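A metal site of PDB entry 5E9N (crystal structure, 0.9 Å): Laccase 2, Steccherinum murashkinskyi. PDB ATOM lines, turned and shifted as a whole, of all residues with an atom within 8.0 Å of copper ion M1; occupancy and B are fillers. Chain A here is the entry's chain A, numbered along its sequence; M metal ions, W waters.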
ATOM      1  N   HIS A  65      -4.179  -2.341   2.988  1.00  0.00           N
ATOM      2  CA  HIS A  65      -5.569  -2.213   3.332  1.00  0.00           C
ATOM      3  C   HIS A  65      -6.253  -3.545   3.152  1.00  0.00           C
ATOM      4  O   HIS A  65      -6.015  -4.301   2.218  1.00  0.00           O
ATOM      5  CB  HIS A  65      -6.203  -1.192   2.432  1.00  0.00           C
ATOM      6  CG  HIS A  65      -7.692  -1.069   2.540  1.00  0.00           C
ATOM      7  ND1 HIS A  65      -8.356  -0.779   3.678  1.00  0.00           N
ATOM      8  CD2 HIS A  65      -8.629  -1.096   1.589  1.00  0.00           C
ATOM      9  CE1 HIS A  65      -9.641  -0.689   3.434  1.00  0.00           C
ATOM     10  NE2 HIS A  65      -9.845  -0.870   2.156  1.00  0.00           N
ATOM     11  N   TRP A  66      -7.178  -3.810   4.078  1.00  0.00           N
ATOM     12  CA  TRP A  66      -7.935  -5.022   4.129  1.00  0.00           C
ATOM     13  C   TRP A  66      -9.296  -4.660   3.660  1.00  0.00           C
ATOM     14  O   TRP A  66     -10.135  -4.129   4.396  1.00  0.00           O
ATOM     15  CB  TRP A  66      -7.874  -5.617   5.595  1.00  0.00           C
ATOM     16  CG  TRP A  66      -6.541  -5.413   6.181  1.00  0.00           C
ATOM     17  CD1 TRP A  66      -6.152  -4.368   6.947  1.00  0.00           C
ATOM     18  CD2 TRP A  66      -5.353  -6.165   5.917  1.00  0.00           C
ATOM     19  NE1 TRP A  66      -4.804  -4.429   7.205  1.00  0.00           N
ATOM     20  CE2 TRP A  66      -4.292  -5.518   6.564  1.00  0.00           C
ATOM     21  CE3 TRP A  66      -5.077  -7.305   5.171  1.00  0.00           C
ATOM     22  CZ2 TRP A  66      -2.989  -5.958   6.465  1.00  0.00           C
ATOM     23  CZ3 TRP A  66      -3.807  -7.744   5.092  1.00  0.00           C
ATOM     24  CH2 TRP A  66      -2.766  -7.092   5.748  1.00  0.00           C
ATOM     25  N   HIS A  67      -9.505  -4.828   2.372  1.00  0.00           N
ATOM     26  CA  HIS A  67     -10.623  -4.222   1.683  1.00  0.00           C
ATOM     27  C   HIS A  67     -11.923  -4.828   2.097  1.00  0.00           C
ATOM     28  O   HIS A  67     -12.176  -5.992   1.895  1.00  0.00           O
ATOM     29  CB  HIS A  67     -10.426  -4.374   0.196  1.00  0.00           C
ATOM     30  CG  HIS A  67     -11.526  -3.758  -0.582  1.00  0.00           C
ATOM     31  ND1 HIS A  67     -11.353  -2.664  -1.388  1.00  0.00           N
ATOM     32  CD2 HIS A  67     -12.852  -4.090  -0.591  1.00  0.00           C
ATOM     33  CE1 HIS A  67     -12.551  -2.388  -1.901  1.00  0.00           C
ATOM     34  NE2 HIS A  67     -13.457  -3.221  -1.424  1.00  0.00           N
ATOM     35  N   GLY A  68     -12.797  -3.966   2.622  1.00  0.00           N
ATOM     36  CA  GLY A  68     -14.120  -4.339   2.983  1.00  0.00           C
ATOM     37  C   GLY A  68     -14.301  -4.690   4.434  1.00  0.00           C
ATOM     38  O   GLY A  68     -15.447  -4.884   4.870  1.00  0.00           O
ATOM     39  N   TRP A 108     -10.417  -8.770   0.039  1.00  0.00           N
ATOM     40  CA  TRP A 108      -9.081  -8.837  -0.535  1.00  0.00           C
ATOM     41  C   TRP A 108      -8.225  -7.827   0.203  1.00  0.00           C
ATOM     42  O   TRP A 108      -8.717  -7.058   0.975  1.00  0.00           O
ATOM     43  CB  TRP A 108      -9.084  -8.653  -2.032  1.00  0.00           C
ATOM     44  CG  TRP A 108      -9.527  -7.346  -2.562  1.00  0.00           C
ATOM     45  CD1 TRP A 108     -10.753  -6.784  -2.486  1.00  0.00           C
ATOM     46  CD2 TRP A 108      -8.764  -6.478  -3.406  1.00  0.00           C
ATOM     47  NE1 TRP A 108     -10.812  -5.644  -3.213  1.00  0.00           N
ATOM     48  CE2 TRP A 108      -9.619  -5.457  -3.827  1.00  0.00           C
ATOM     49  CE3 TRP A 108      -7.445  -6.521  -3.891  1.00  0.00           C
ATOM     50  CZ2 TRP A 108      -9.170  -4.457  -4.672  1.00  0.00           C
ATOM     51  CZ3 TRP A 108      -7.046  -5.545  -4.750  1.00  0.00           C
ATOM     52  CH2 TRP A 108      -7.893  -4.529  -5.150  1.00  0.00           C
ATOM     53  N   TYR A 109      -6.941  -7.913  -0.034  1.00  0.00           N
ATOM     54  CA  TYR A 109      -5.991  -6.982   0.567  1.00  0.00           C
ATOM     55  C   TYR A 109      -5.122  -6.445  -0.533  1.00  0.00           C
ATOM     56  O   TYR A 109      -4.866  -7.098  -1.543  1.00  0.00           O
ATOM     57  CB  TYR A 109      -5.151  -7.639   1.660  1.00  0.00           C
ATOM     58  CG  TYR A 109      -4.257  -8.735   1.218  1.00  0.00           C
ATOM     59  CD1 TYR A 109      -2.946  -8.518   0.862  1.00  0.00           C
ATOM     60  CD2 TYR A 109      -4.710 -10.036   1.132  1.00  0.00           C
ATOM     61  CE1 TYR A 109      -2.128  -9.525   0.450  1.00  0.00           C
ATOM     62  CE2 TYR A 109      -3.912 -11.069   0.737  1.00  0.00           C
ATOM     63  CZ  TYR A 109      -2.599 -10.810   0.393  1.00  0.00           C
ATOM     64  OH  TYR A 109      -1.755 -11.806  -0.018  1.00  0.00           O
ATOM     65  N   HIS A 110      -4.635  -5.247  -0.318  1.00  0.00           N
ATOM     66  CA  HIS A 110      -3.835  -4.595  -1.327  1.00  0.00           C
ATOM     67  C   HIS A 110      -3.056  -3.487  -0.729  1.00  0.00           C
ATOM     68  O   HIS A 110      -3.447  -2.860   0.254  1.00  0.00           O
ATOM     69  CB  HIS A 110      -4.671  -4.116  -2.486  1.00  0.00           C
ATOM     70  CG  HIS A 110      -5.787  -3.180  -2.162  1.00  0.00           C
ATOM     71  ND1 HIS A 110      -5.627  -1.833  -2.018  1.00  0.00           N
ATOM     72  CD2 HIS A 110      -7.115  -3.413  -2.017  1.00  0.00           C
ATOM     73  CE1 HIS A 110      -6.831  -1.285  -1.821  1.00  0.00           C
ATOM     74  NE2 HIS A 110      -7.751  -2.214  -1.829  1.00  0.00           N
ATOM     75  N   SER A 111      -1.922  -3.172  -1.372  1.00  0.00           N
ATOM     76  CA  SER A 111      -1.250  -1.941  -0.996  1.00  0.00           C
ATOM     77  C   SER A 111      -2.213  -0.771  -1.116  1.00  0.00           C
ATOM     78  O   SER A 111      -3.040  -0.722  -2.029  1.00  0.00           O
ATOM     79  CB  SER A 111      -0.075  -1.659  -1.898  1.00  0.00           C
ATOM     80  OG  SER A 111       0.517  -0.467  -1.467  1.00  0.00           O
ATOM     81  N   HIS A 112      -2.066   0.170  -0.206  1.00  0.00           N
ATOM     82  CA  HIS A 112      -2.846   1.388  -0.235  1.00  0.00           C
ATOM     83  C   HIS A 112      -1.933   2.580  -0.119  1.00  0.00           C
ATOM     84  O   HIS A 112      -2.258   3.571   0.549  1.00  0.00           O
ATOM     85  CB  HIS A 112      -3.970   1.357   0.798  1.00  0.00           C
ATOM     86  CG  HIS A 112      -5.175   2.106   0.400  1.00  0.00           C
ATOM     87  ND1 HIS A 112      -5.173   3.352  -0.119  1.00  0.00           N
ATOM     88  CD2 HIS A 112      -6.476   1.755   0.402  1.00  0.00           C
ATOM     89  CE1 HIS A 112      -6.419   3.696  -0.412  1.00  0.00           C
ATOM     90  NE2 HIS A 112      -7.265   2.714  -0.107  1.00  0.00           N
ATOM     91  N   TYR A 117      -0.375  -1.074  -5.470  1.00  0.00           N
ATOM     92  CA  TYR A 117      -0.985  -2.370  -5.605  1.00  0.00           C
ATOM     93  C   TYR A 117      -0.961  -2.825  -7.042  1.00  0.00           C
ATOM     94  O   TYR A 117      -0.947  -4.025  -7.311  1.00  0.00           O
ATOM     95  CB  TYR A 117      -2.350  -2.499  -4.948  1.00  0.00           C
ATOM     96  CG  TYR A 117      -3.622  -2.124  -5.662  1.00  0.00           C
ATOM     97  CD1 TYR A 117      -4.195  -2.957  -6.621  1.00  0.00           C
ATOM     98  CD2 TYR A 117      -4.388  -1.060  -5.265  1.00  0.00           C
ATOM     99  CE1 TYR A 117      -5.421  -2.702  -7.166  1.00  0.00           C
ATOM    100  CE2 TYR A 117      -5.618  -0.816  -5.791  1.00  0.00           C
ATOM    101  CZ  TYR A 117      -6.156  -1.639  -6.738  1.00  0.00           C
ATOM    102  OH  TYR A 117      -7.388  -1.333  -7.211  1.00  0.00           O
ATOM    103  N   SER A 205     -12.352  -9.201  -7.959  1.00  0.00           N
ATOM    104  CA  SER A 205     -11.646  -8.281  -8.784  1.00  0.00           C
ATOM    105  C   SER A 205     -10.561  -7.609  -7.974  1.00  0.00           C
ATOM    106  O   SER A 205     -10.861  -6.851  -7.053  1.00  0.00           O
ATOM    107  CB  SER A 205     -12.530  -7.211  -9.354  1.00  0.00           C
ATOM    108  OG  SER A 205     -11.678  -6.238  -9.930  1.00  0.00           O
ATOM    109  N   ILE A 206      -9.316  -7.909  -8.331  1.00  0.00           N
ATOM    110  CA  ILE A 206      -8.172  -7.215  -7.748  1.00  0.00           C
ATOM    111  C   ILE A 206      -7.652  -6.210  -8.750  1.00  0.00           C
ATOM    112  O   ILE A 206      -6.493  -5.841  -8.749  1.00  0.00           O
ATOM    113  CB  ILE A 206      -7.121  -8.181  -7.236  1.00  0.00           C
ATOM    114  CG1 ILE A 206      -6.512  -9.048  -8.345  1.00  0.00           C
ATOM    115  CG2 ILE A 206      -7.744  -9.078  -6.175  1.00  0.00           C
ATOM    116  CD1 ILE A 206      -5.456  -9.972  -7.861  1.00  0.00           C
ATOM    117  N   SER A 207      -8.525  -5.713  -9.610  1.00  0.00           N
ATOM    118  CA  SER A 207      -8.150  -4.793 -10.652  1.00  0.00           C
ATOM    119  C   SER A 207      -7.735  -3.429 -10.094  1.00  0.00           C
ATOM    120  O   SER A 207      -8.338  -2.927  -9.157  1.00  0.00           O
ATOM    121  CB  SER A 207      -9.370  -4.596 -11.560  1.00  0.00           C
ATOM    122  OG  SER A 207      -9.027  -3.801 -12.648  1.00  0.00           O
ATOM    123  N   ALA A 243     -13.736  -2.861 -10.464  1.00  0.00           N
ATOM    124  CA  ALA A 243     -12.542  -2.992  -9.645  1.00  0.00           C
ATOM    125  C   ALA A 243     -12.930  -3.058  -8.185  1.00  0.00           C
ATOM    126  O   ALA A 243     -13.689  -2.234  -7.705  1.00  0.00           O
ATOM    127  CB  ALA A 243     -11.626  -1.804  -9.889  1.00  0.00           C
ATOM    128  N   ALA A 244     -12.351  -4.048  -7.507  1.00  0.00           N
ATOM    129  CA  ALA A 244     -12.452  -4.235  -6.075  1.00  0.00           C
ATOM    130  C   ALA A 244     -13.716  -4.942  -5.603  1.00  0.00           C
ATOM    131  O   ALA A 244     -13.800  -5.259  -4.425  1.00  0.00           O
ATOM    132  CB  ALA A 244     -12.272  -2.970  -5.283  1.00  0.00           C
ATOM    133  N   GLN A 245     -14.648  -5.217  -6.491  1.00  0.00           N
ATOM    134  CA  GLN A 245     -15.849  -5.939  -6.146  1.00  0.00           C
ATOM    135  C   GLN A 245     -15.564  -7.405  -5.990  1.00  0.00           C
ATOM    136  O   GLN A 245     -14.583  -7.932  -6.518  1.00  0.00           O
ATOM    137  CB  GLN A 245     -16.916  -5.714  -7.195  1.00  0.00           C
ATOM    138  CG  GLN A 245     -17.454  -4.317  -7.196  1.00  0.00           C
ATOM    139  CD  GLN A 245     -18.530  -4.112  -8.207  1.00  0.00           C
ATOM    140  OE1 GLN A 245     -18.601  -4.820  -9.216  1.00  0.00           O
ATOM    141  NE2 GLN A 245     -19.397  -3.142  -7.968  1.00  0.00           N
ATOM    142  N   ARG A 246     -16.484  -8.073  -5.288  1.00  0.00           N
ATOM    143  CA  ARG A 246     -16.444  -9.514  -5.174  1.00  0.00           C
ATOM    144  C   ARG A 246     -17.851 -10.065  -5.324  1.00  0.00           C
ATOM    145  O   ARG A 246     -18.823  -9.461  -4.893  1.00  0.00           O
ATOM    146  CB  ARG A 246     -15.919  -9.980  -3.820  1.00  0.00           C
ATOM    147  CG  ARG A 246     -14.450  -9.636  -3.573  1.00  0.00           C
ATOM    148  CD  ARG A 246     -14.197  -8.232  -3.102  1.00  0.00           C
ATOM    149  NE  ARG A 246     -14.820  -8.017  -1.805  1.00  0.00           N
ATOM    150  CZ  ARG A 246     -15.368  -6.903  -1.385  1.00  0.00           C
ATOM    151  NH1 ARG A 246     -15.371  -5.815  -2.110  1.00  0.00           N
ATOM    152  NH2 ARG A 246     -15.944  -6.900  -0.202  1.00  0.00           N
ATOM    153  N   HIS A 400     -15.757   3.320  -3.679  1.00  0.00           N
ATOM    154  CA  HIS A 400     -15.588   2.450  -2.547  1.00  0.00           C
ATOM    155  C   HIS A 400     -15.476   3.301  -1.301  1.00  0.00           C
ATOM    156  O   HIS A 400     -14.817   4.300  -1.284  1.00  0.00           O
ATOM    157  CB  HIS A 400     -14.331   1.628  -2.730  1.00  0.00           C
ATOM    158  CG  HIS A 400     -13.920   0.881  -1.522  1.00  0.00           C
ATOM    159  ND1 HIS A 400     -14.731  -0.025  -0.882  1.00  0.00           N
ATOM    160  CD2 HIS A 400     -12.777   0.892  -0.832  1.00  0.00           C
ATOM    161  CE1 HIS A 400     -14.095  -0.512   0.156  1.00  0.00           C
ATOM    162  NE2 HIS A 400     -12.899   0.031   0.225  1.00  0.00           N
ATOM    163  N   HIS A 402     -14.465   2.952   2.747  1.00  0.00           N
ATOM    164  CA  HIS A 402     -13.873   2.192   3.824  1.00  0.00           C
ATOM    165  C   HIS A 402     -14.780   2.192   5.040  1.00  0.00           C
ATOM    166  O   HIS A 402     -15.627   3.062   5.216  1.00  0.00           O
ATOM    167  CB  HIS A 402     -12.543   2.789   4.203  1.00  0.00           C
ATOM    168  CG  HIS A 402     -11.464   2.666   3.192  1.00  0.00           C
ATOM    169  ND1 HIS A 402     -10.184   2.431   3.591  1.00  0.00           N
ATOM    170  CD2 HIS A 402     -11.404   2.777   1.846  1.00  0.00           C
ATOM    171  CE1 HIS A 402      -9.393   2.389   2.528  1.00  0.00           C
ATOM    172  NE2 HIS A 402     -10.103   2.629   1.447  1.00  0.00           N
ATOM    173  N   ASP A 426     -19.790  -2.772  -0.923  1.00  0.00           N
ATOM    174  CA  ASP A 426     -18.818  -1.775  -0.529  1.00  0.00           C
ATOM    175  C   ASP A 426     -18.146  -1.049  -1.673  1.00  0.00           C
ATOM    176  O   ASP A 426     -17.469  -0.058  -1.415  1.00  0.00           O
ATOM    177  CB  ASP A 426     -17.781  -2.336   0.447  1.00  0.00           C
ATOM    178  CG  ASP A 426     -16.858  -3.362  -0.091  1.00  0.00           C
ATOM    179  OD1 ASP A 426     -16.624  -4.362   0.649  1.00  0.00           O
ATOM    180  OD2 ASP A 426     -16.367  -3.210  -1.233  1.00  0.00           O
ATOM    181  N   THR A 427     -18.364  -1.504  -2.901  1.00  0.00           N
ATOM    182  CA  THR A 427     -17.781  -0.852  -4.072  1.00  0.00           C
ATOM    183  C   THR A 427     -18.858  -0.867  -5.130  1.00  0.00           C
ATOM    184  O   THR A 427     -19.387  -1.920  -5.402  1.00  0.00           O
ATOM    185  CB  THR A 427     -16.546  -1.588  -4.544  1.00  0.00           C
ATOM    186  OG1 THR A 427     -15.605  -1.655  -3.466  1.00  0.00           O
ATOM    187  CG2 THR A 427     -15.910  -0.935  -5.712  1.00  0.00           C
ATOM    188  N   HIS A 452     -13.460   6.751  -2.284  1.00  0.00           N
ATOM    189  CA  HIS A 452     -12.713   7.051  -3.488  1.00  0.00           C
ATOM    190  C   HIS A 452     -13.118   6.136  -4.602  1.00  0.00           C
ATOM    191  O   HIS A 452     -13.605   5.044  -4.403  1.00  0.00           O
ATOM    192  CB  HIS A 452     -11.225   6.964  -3.255  1.00  0.00           C
ATOM    193  CG  HIS A 452     -10.728   5.622  -2.823  1.00  0.00           C
ATOM    194  ND1 HIS A 452     -10.340   4.663  -3.717  1.00  0.00           N
ATOM    195  CD2 HIS A 452     -10.529   5.088  -1.608  1.00  0.00           C
ATOM    196  CE1 HIS A 452      -9.939   3.587  -3.041  1.00  0.00           C
ATOM    197  NE2 HIS A 452     -10.017   3.813  -1.745  1.00  0.00           N
ATOM    198  N   HIS A 454     -12.107   3.370  -6.996  1.00  0.00           N
ATOM    199  CA  HIS A 454     -11.141   2.304  -6.842  1.00  0.00           C
ATOM    200  C   HIS A 454     -10.357   2.009  -8.094  1.00  0.00           C
ATOM    201  O   HIS A 454      -9.534   1.126  -8.071  1.00  0.00           O
ATOM    202  CB  HIS A 454     -11.817   1.048  -6.287  1.00  0.00           C
ATOM    203  CG  HIS A 454     -10.936   0.279  -5.366  1.00  0.00           C
ATOM    204  ND1 HIS A 454      -9.761  -0.314  -5.736  1.00  0.00           N
ATOM    205  CD2 HIS A 454     -11.093  -0.052  -4.053  1.00  0.00           C
ATOM    206  CE1 HIS A 454      -9.236  -0.903  -4.667  1.00  0.00           C
ATOM    207  NE2 HIS A 454     -10.031  -0.784  -3.622  1.00  0.00           N
ATOM    208  N   ASP A 456      -7.252   2.777  -9.502  1.00  0.00           N
ATOM    209  CA  ASP A 456      -6.155   3.275  -8.688  1.00  0.00           C
ATOM    210  C   ASP A 456      -5.533   4.490  -9.327  1.00  0.00           C
ATOM    211  O   ASP A 456      -5.065   5.415  -8.631  1.00  0.00           O
ATOM    212  CB  ASP A 456      -5.140   2.176  -8.442  1.00  0.00           C
ATOM    213  CG  ASP A 456      -4.532   2.284  -7.045  1.00  0.00           C
ATOM    214  OD1 ASP A 456      -5.185   2.707  -6.082  1.00  0.00           O
ATOM    215  OD2 ASP A 456      -3.371   1.861  -6.909  1.00  0.00           O
HETATM  216 CU    CU M   1      -9.693  -2.025  -2.003  1.00  0.00          CU
HETATM  217 CU    CU M   2     -11.481  -0.489   1.323  1.00  0.00          CU
HETATM  218 CU    CU M   3      -9.229   2.963  -0.260  1.00  0.00          CU
HETATM  219  O   HOH W   1      -9.285   0.700  -1.250  1.00  0.00           O
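The side-chain hydroxyl (OH) of Tyr 117 is in hydrogen-bond range of a ring nitrogen (ND1) of His 454, 3.0 Å away.
N of His 65 lies within hydrogen-bond range of O of His 110.
NE2 of His 67 sits at hydrogen-bond distance from OD2 of Asp 426, 2.9 Å away.
O of Trp 108 lies within hydrogen-bond range of N of His 67.
NE1 of Trp 108 is in hydrogen-bond range of O of Ala 244.
A ring nitrogen (NE2) of His 67 lies within hydrogen-bond range of the guanidinium group (NH1) of Arg 246 (3.3 Å).
A ring nitrogen (NE2) of His 67 lies within hydrogen-bond range of the side-chain hydroxyl (OG1) of Thr 427 (3.4 Å).
NE2 of His 67 lies close to ND1 of His 400, 3.5 Å away.
CD2 of His 65 touches copper ion M1, 3.9 Å away.
Trp 108 touches copper ion M1 (CZ2 to CU, 3.6 Å).
Copper ion M1 is bound by a ring nitrogen (ND1) of His 67 (1.9 Å), a ring nitrogen (NE2) of His 110 (2.0 Å) and a ring nitrogen (NE2) of His 454 (2.1 Å).
Copper ion M1 has three donor atoms within binding distance.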
